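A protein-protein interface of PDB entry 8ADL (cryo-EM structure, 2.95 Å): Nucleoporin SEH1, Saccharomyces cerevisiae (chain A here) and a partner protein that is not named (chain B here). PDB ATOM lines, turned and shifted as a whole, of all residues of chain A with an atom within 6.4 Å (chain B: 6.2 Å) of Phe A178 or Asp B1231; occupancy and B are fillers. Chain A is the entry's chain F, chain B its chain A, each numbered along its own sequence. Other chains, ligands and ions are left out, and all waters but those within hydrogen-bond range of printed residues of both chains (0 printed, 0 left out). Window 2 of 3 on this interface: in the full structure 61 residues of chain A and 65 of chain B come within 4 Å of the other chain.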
ATOM      1  N   HIS A 120      12.086  16.579   2.577  1.00  0.00           N
ATOM      2  CA  HIS A 120      12.004  17.723   1.680  1.00  0.00           C
ATOM      3  C   HIS A 120      10.982  18.759   2.130  1.00  0.00           C
ATOM      4  O   HIS A 120      10.849  19.798   1.475  1.00  0.00           O
ATOM      5  CB  HIS A 120      11.696  17.257   0.255  1.00  0.00           C
ATOM      6  CG  HIS A 120      10.293  16.775   0.060  1.00  0.00           C
ATOM      7  ND1 HIS A 120       9.307  17.558  -0.500  1.00  0.00           N
ATOM      8  CD2 HIS A 120       9.712  15.584   0.342  1.00  0.00           C
ATOM      9  CE1 HIS A 120       8.179  16.872  -0.551  1.00  0.00           C
ATOM     10  NE2 HIS A 120       8.398  15.671  -0.047  1.00  0.00           N
ATOM     11  N   PRO A 175       5.460  10.018   1.067  1.00  0.00           N
ATOM     12  CA  PRO A 175       6.876  10.254   0.765  1.00  0.00           C
ATOM     13  C   PRO A 175       7.157  10.742  -0.649  1.00  0.00           C
ATOM     14  O   PRO A 175       8.322  10.743  -1.056  1.00  0.00           O
ATOM     15  CB  PRO A 175       7.516   8.871   0.995  1.00  0.00           C
ATOM     16  CG  PRO A 175       6.420   7.977   1.515  1.00  0.00           C
ATOM     17  CD  PRO A 175       5.139   8.586   1.082  1.00  0.00           C
ATOM     18  N   SER A 176       6.141  11.144  -1.408  1.00  0.00           N
ATOM     19  CA  SER A 176       6.356  11.631  -2.765  1.00  0.00           C
ATOM     20  C   SER A 176       6.977  13.022  -2.709  1.00  0.00           C
ATOM     21  O   SER A 176       6.378  13.954  -2.161  1.00  0.00           O
ATOM     22  CB  SER A 176       5.037  11.651  -3.531  1.00  0.00           C
ATOM     23  OG  SER A 176       5.238  11.899  -4.908  1.00  0.00           O
ATOM     24  N   ARG A 177       8.179  13.161  -3.273  1.00  0.00           N
ATOM     25  CA  ARG A 177       8.920  14.413  -3.139  1.00  0.00           C
ATOM     26  C   ARG A 177       8.334  15.525  -4.002  1.00  0.00           C
ATOM     27  O   ARG A 177       8.437  16.703  -3.642  1.00  0.00           O
ATOM     28  CB  ARG A 177      10.392  14.185  -3.488  1.00  0.00           C
ATOM     29  CG  ARG A 177      11.318  15.317  -3.067  1.00  0.00           C
ATOM     30  CD  ARG A 177      12.778  14.910  -3.140  1.00  0.00           C
ATOM     31  NE  ARG A 177      13.150  14.012  -2.055  1.00  0.00           N
ATOM     32  CZ  ARG A 177      14.353  13.970  -1.498  1.00  0.00           C
ATOM     33  NH1 ARG A 177      15.331  14.762  -1.907  1.00  0.00           N
ATOM     34  NH2 ARG A 177      14.581  13.114  -0.507  1.00  0.00           N
ATOM     35  N   PHE A 178       7.711  15.182  -5.126  1.00  0.00           N
ATOM     36  CA  PHE A 178       7.271  16.187  -6.082  1.00  0.00           C
ATOM     37  C   PHE A 178       5.762  16.267  -6.238  1.00  0.00           C
ATOM     38  O   PHE A 178       5.276  17.185  -6.909  1.00  0.00           O
ATOM     39  CB  PHE A 178       7.933  15.933  -7.442  1.00  0.00           C
ATOM     40  CG  PHE A 178       9.431  15.977  -7.388  1.00  0.00           C
ATOM     41  CD1 PHE A 178      10.100  17.185  -7.482  1.00  0.00           C
ATOM     42  CD2 PHE A 178      10.171  14.820  -7.197  1.00  0.00           C
ATOM     43  CE1 PHE A 178      11.475  17.235  -7.418  1.00  0.00           C
ATOM     44  CE2 PHE A 178      11.548  14.865  -7.125  1.00  0.00           C
ATOM     45  CZ  PHE A 178      12.201  16.073  -7.238  1.00  0.00           C
ATOM     46  N   SER A 179       5.014  15.345  -5.648  1.00  0.00           N
ATOM     47  CA  SER A 179       3.586  15.534  -5.482  1.00  0.00           C
ATOM     48  C   SER A 179       3.335  16.524  -4.348  1.00  0.00           C
ATOM     49  O   SER A 179       4.219  16.765  -3.521  1.00  0.00           O
ATOM     50  CB  SER A 179       2.908  14.199  -5.187  1.00  0.00           C
ATOM     51  OG  SER A 179       3.151  13.265  -6.225  1.00  0.00           O
ATOM     52  N   PRO A 180       2.153  17.144  -4.308  1.00  0.00           N
ATOM     53  CA  PRO A 180       1.815  18.008  -3.173  1.00  0.00           C
ATOM     54  C   PRO A 180       1.760  17.239  -1.860  1.00  0.00           C
ATOM     55  O   PRO A 180       1.589  16.019  -1.826  1.00  0.00           O
ATOM     56  CB  PRO A 180       0.438  18.564  -3.546  1.00  0.00           C
ATOM     57  CG  PRO A 180       0.428  18.560  -5.024  1.00  0.00           C
ATOM     58  CD  PRO A 180       1.276  17.398  -5.467  1.00  0.00           C
ATOM     59  N   ILE B1197       6.402  14.150 -15.459  1.00  0.00           N
ATOM     60  CA  ILE B1197       7.702  14.523 -14.912  1.00  0.00           C
ATOM     61  C   ILE B1197       7.722  14.342 -13.398  1.00  0.00           C
ATOM     62  O   ILE B1197       8.762  13.997 -12.820  1.00  0.00           O
ATOM     63  CB  ILE B1197       8.038  15.969 -15.328  1.00  0.00           C
ATOM     64  CG1 ILE B1197       7.942  16.119 -16.845  1.00  0.00           C
ATOM     65  CG2 ILE B1197       9.441  16.359 -14.894  1.00  0.00           C
ATOM     66  CD1 ILE B1197       8.911  15.248 -17.608  1.00  0.00           C
ATOM     67  N   ASP B1198       6.572  14.528 -12.740  1.00  0.00           N
ATOM     68  CA  ASP B1198       6.485  14.350 -11.293  1.00  0.00           C
ATOM     69  C   ASP B1198       6.747  12.904 -10.890  1.00  0.00           C
ATOM     70  O   ASP B1198       7.508  12.642  -9.953  1.00  0.00           O
ATOM     71  CB  ASP B1198       5.116  14.806 -10.792  1.00  0.00           C
ATOM     72  CG  ASP B1198       4.837  16.264 -11.104  1.00  0.00           C
ATOM     73  OD1 ASP B1198       5.717  16.927 -11.691  1.00  0.00           O
ATOM     74  OD2 ASP B1198       3.737  16.745 -10.761  1.00  0.00           O
ATOM     75  N   ILE B1199       6.140  11.951 -11.603  1.00  0.00           N
ATOM     76  CA  ILE B1199       6.302  10.537 -11.272  1.00  0.00           C
ATOM     77  C   ILE B1199       7.735  10.083 -11.531  1.00  0.00           C
ATOM     78  O   ILE B1199       8.324   9.350 -10.724  1.00  0.00           O
ATOM     79  CB  ILE B1199       5.284   9.693 -12.060  1.00  0.00           C
ATOM     80  CG1 ILE B1199       3.860  10.166 -11.759  1.00  0.00           C
ATOM     81  CG2 ILE B1199       5.430   8.216 -11.729  1.00  0.00           C
ATOM     82  CD1 ILE B1199       2.790   9.399 -12.503  1.00  0.00           C
ATOM     83  N   LYS B1201      10.507  12.012 -11.593  1.00  0.00           N
ATOM     84  CA  LYS B1201      11.390  12.641 -10.619  1.00  0.00           C
ATOM     85  C   LYS B1201      11.218  12.025  -9.235  1.00  0.00           C
ATOM     86  O   LYS B1201      12.195  11.879  -8.492  1.00  0.00           O
ATOM     87  CB  LYS B1201      11.140  14.147 -10.576  1.00  0.00           C
ATOM     88  CG  LYS B1201      11.737  14.922 -11.736  1.00  0.00           C
ATOM     89  CD  LYS B1201      11.930  16.383 -11.361  1.00  0.00           C
ATOM     90  CE  LYS B1201      10.633  17.164 -11.471  1.00  0.00           C
ATOM     91  NZ  LYS B1201      10.860  18.631 -11.369  1.00  0.00           N
ATOM     92  N   ASP B1202       9.987  11.640  -8.879  1.00  0.00           N
ATOM     93  CA  ASP B1202       9.754  10.966  -7.605  1.00  0.00           C
ATOM     94  C   ASP B1202      10.413   9.595  -7.578  1.00  0.00           C
ATOM     95  O   ASP B1202      10.951   9.185  -6.543  1.00  0.00           O
ATOM     96  CB  ASP B1202       8.255  10.832  -7.351  1.00  0.00           C
ATOM     97  CG  ASP B1202       7.651  12.089  -6.774  1.00  0.00           C
ATOM     98  OD1 ASP B1202       8.261  12.670  -5.856  1.00  0.00           O
ATOM     99  OD2 ASP B1202       6.558  12.491  -7.225  1.00  0.00           O
ATOM    100  N   ALA B1203      10.378   8.874  -8.701  1.00  0.00           N
ATOM    101  CA  ALA B1203      11.043   7.577  -8.768  1.00  0.00           C
ATOM    102  C   ALA B1203      12.554   7.722  -8.645  1.00  0.00           C
ATOM    103  O   ALA B1203      13.202   6.926  -7.953  1.00  0.00           O
ATOM    104  CB  ALA B1203      10.677   6.865 -10.065  1.00  0.00           C
ATOM    105  N   ALA B1205      14.121  10.206  -7.128  1.00  0.00           N
ATOM    106  CA  ALA B1205      14.380  10.616  -5.751  1.00  0.00           C
ATOM    107  C   ALA B1205      14.281   9.439  -4.786  1.00  0.00           C
ATOM    108  O   ALA B1205      15.089   9.321  -3.858  1.00  0.00           O
ATOM    109  CB  ALA B1205      13.412  11.725  -5.343  1.00  0.00           C
ATOM    110  N   PHE B1229      17.308  15.467 -14.841  1.00  0.00           N
ATOM    111  CA  PHE B1229      16.437  16.325 -14.050  1.00  0.00           C
ATOM    112  C   PHE B1229      17.290  17.057 -13.021  1.00  0.00           C
ATOM    113  O   PHE B1229      17.953  16.423 -12.194  1.00  0.00           O
ATOM    114  CB  PHE B1229      15.339  15.507 -13.374  1.00  0.00           C
ATOM    115  CG  PHE B1229      14.812  14.382 -14.220  1.00  0.00           C
ATOM    116  CD1 PHE B1229      13.944  14.634 -15.269  1.00  0.00           C
ATOM    117  CD2 PHE B1229      15.185  13.071 -13.964  1.00  0.00           C
ATOM    118  CE1 PHE B1229      13.458  13.601 -16.050  1.00  0.00           C
ATOM    119  CE2 PHE B1229      14.704  12.034 -14.742  1.00  0.00           C
ATOM    120  CZ  PHE B1229      13.840  12.300 -15.784  1.00  0.00           C
ATOM    121  N   GLU B1230      17.271  18.388 -13.072  1.00  0.00           N
ATOM    122  CA  GLU B1230      18.233  19.201 -12.339  1.00  0.00           C
ATOM    123  C   GLU B1230      17.825  19.492 -10.901  1.00  0.00           C
ATOM    124  O   GLU B1230      18.633  20.046 -10.149  1.00  0.00           O
ATOM    125  CB  GLU B1230      18.463  20.524 -13.075  1.00  0.00           C
ATOM    126  CG  GLU B1230      17.236  21.419 -13.135  1.00  0.00           C
ATOM    127  CD  GLU B1230      16.468  21.268 -14.434  1.00  0.00           C
ATOM    128  OE1 GLU B1230      16.925  20.505 -15.311  1.00  0.00           O
ATOM    129  OE2 GLU B1230      15.406  21.909 -14.576  1.00  0.00           O
ATOM    130  N   ASP B1231      16.607  19.142 -10.498  1.00  0.00           N
ATOM    131  CA  ASP B1231      16.072  19.527  -9.196  1.00  0.00           C
ATOM    132  C   ASP B1231      15.555  18.286  -8.466  1.00  0.00           C
ATOM    133  O   ASP B1231      14.430  18.234  -7.967  1.00  0.00           O
ATOM    134  CB  ASP B1231      15.004  20.610  -9.387  1.00  0.00           C
ATOM    135  CG  ASP B1231      14.506  21.201  -8.073  1.00  0.00           C
ATOM    136  OD1 ASP B1231      15.254  21.987  -7.456  1.00  0.00           O
ATOM    137  OD2 ASP B1231      13.366  20.891  -7.669  1.00  0.00           O
ATOM    138  N   ILE B1232      16.377  17.240  -8.424  1.00  0.00           N
ATOM    139  CA  ILE B1232      15.955  15.988  -7.800  1.00  0.00           C
ATOM    140  C   ILE B1232      16.115  16.057  -6.287  1.00  0.00           C
ATOM    141  O   ILE B1232      15.143  15.912  -5.535  1.00  0.00           O
ATOM    142  CB  ILE B1232      16.731  14.800  -8.394  1.00  0.00           C
ATOM    143  CG1 ILE B1232      16.307  14.561  -9.843  1.00  0.00           C
ATOM    144  CG2 ILE B1232      16.496  13.544  -7.568  1.00  0.00           C
ATOM    145  CD1 ILE B1232      14.898  14.027  -9.988  1.00  0.00           C
ATOM    146  N   MET B1233      17.339  16.283  -5.815  1.00  0.00           N
ATOM    147  CA  MET B1233      17.637  16.338  -4.388  1.00  0.00           C
ATOM    148  C   MET B1233      18.115  17.744  -4.051  1.00  0.00           C
ATOM    149  O   MET B1233      19.250  18.113  -4.374  1.00  0.00           O
ATOM    150  CB  MET B1233      18.681  15.291  -4.003  1.00  0.00           C
ATOM    151  CG  MET B1233      18.093  13.916  -3.726  1.00  0.00           C
ATOM    152  SD  MET B1233      19.157  12.877  -2.711  1.00  0.00           S
ATOM    153  CE  MET B1233      20.428  12.439  -3.894  1.00  0.00           C
ATOM    154  N   GLY B1234      17.256  18.519  -3.409  1.00  0.00           N
ATOM    155  CA  GLY B1234      17.604  19.883  -3.046  1.00  0.00           C
ATOM    156  C   GLY B1234      17.194  20.883  -4.108  1.00  0.00           C
ATOM    157  O   GLY B1234      17.204  20.608  -5.307  1.00  0.00           O
ATOM    158  N   SER B1235      16.825  22.078  -3.647  1.00  0.00           N
ATOM    159  CA  SER B1235      16.439  23.169  -4.534  1.00  0.00           C
ATOM    160  C   SER B1235      17.281  24.421  -4.324  1.00  0.00           C
ATOM    161  O   SER B1235      16.972  25.466  -4.908  1.00  0.00           O
ATOM    162  CB  SER B1235      14.955  23.501  -4.353  1.00  0.00           C
ATOM    163  OG  SER B1235      14.533  24.478  -5.289  1.00  0.00           O
ATOM    164  N   GLU B1236      18.329  24.347  -3.510  1.00  0.00           N
ATOM    165  CA  GLU B1236      19.188  25.492  -3.244  1.00  0.00           C
ATOM    166  C   GLU B1236      20.369  25.582  -4.201  1.00  0.00           C
ATOM    167  O   GLU B1236      21.199  26.485  -4.054  1.00  0.00           O
ATOM    168  CB  GLU B1236      19.699  25.444  -1.800  1.00  0.00           C
ATOM    169  CG  GLU B1236      18.604  25.529  -0.751  1.00  0.00           C
ATOM    170  CD  GLU B1236      17.949  26.894  -0.699  1.00  0.00           C
ATOM    171  OE1 GLU B1236      18.653  27.902  -0.922  1.00  0.00           O
ATOM    172  OE2 GLU B1236      16.730  26.961  -0.436  1.00  0.00           O
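The side-chain hydroxyl (OG) of Ser A176 sits at hydrogen-bond distance from the side-chain carboxylate (OD2) of Asp B1202, at 2.7 Å. N of Phe A178 lies within hydrogen-bond range of OD1 of Asp B1202, 2.7 Å away. OD1 of Asp B1202 is in hydrogen-bond range of N of Arg A177, at 2.6 Å.
The backbone carbonyl oxygen of Arg A177 lies close to a ring nitrogen (ND1) of His A120, at 3.4 Å. A ring nitrogen (NE2) of His A120 is in hydrogen-bond range of the backbone carbonyl oxygen (O) of Ser A176, at 3.4 Å. The side-chain carboxylate (OD1) of Asp B1231 lies close to the side-chain hydroxyl (OG) of Ser B1235 (3.4 Å). The side-chain hydroxyl of Ser A179 sits at hydrogen-bond distance from the side-chain hydroxyl of Ser A176, at 2.8 Å.
Arg A177 touches Ala B1205. CD of Arg A177 touches O of Ile B1232, 3.5 Å away. Arg A177 touches Met B1233 (NH1 to CG, 3.4 Å). O of Lys B1201 touches CE2 of Phe A178, 3.3 Å away. Phe A178 touches Asp B1231 (CE1 to O, 3.2 Å). CZ of Phe A178 touches O of Ile B1232, 3.4 Å away. OD2 of Asp B1202 touches N of Ser A179, 3.6 Å away.
Printed residues of chain B within 4 Å of Arg A177: Asp B1202 (2.6 Å), Ala B1205 (3.9 Å), Ile B1232 (3.5 Å) and Met B1233 (3.4 Å). Of chain B, only Lys B1201, Asp B1202, Asp B1231 and Ile B1232 come within 4 Å of Phe A178. Of the printed residues of chain B, Ser A179 touches Asp B1202. Pro A180 touches none of the printed residues of chain B. Of the printed residues of chain A, Lys B1201 touches Phe A178 (3.3 Å). Asp B1231 touches just one residue of chain A: Phe A178. Of the printed residues of chain A, Met B1233 touches Arg A177. Gly B1234 touches none of the printed residues of chain A. The nearest residue of chain B that does not touch Phe A178 is Ala B1205 (4.1 Å).
Of the 15 printed residues of chain B, 6 touch a printed residue of chain A. Hydrophobic or aromatic side chains of chain B within 4 Å of the printed part of chain A: Ala B1205 and Met B1233. Hydrophobic or aromatic side chains of chain A within 4 Å of the printed part of chain B: Phe A178. Among the printed residues, 10 pairs touch across the chains. Among the printed residues, no Asp or Glu carboxylate lies within 4 Å of a Lys or Arg side-chain nitrogen of the other chain.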
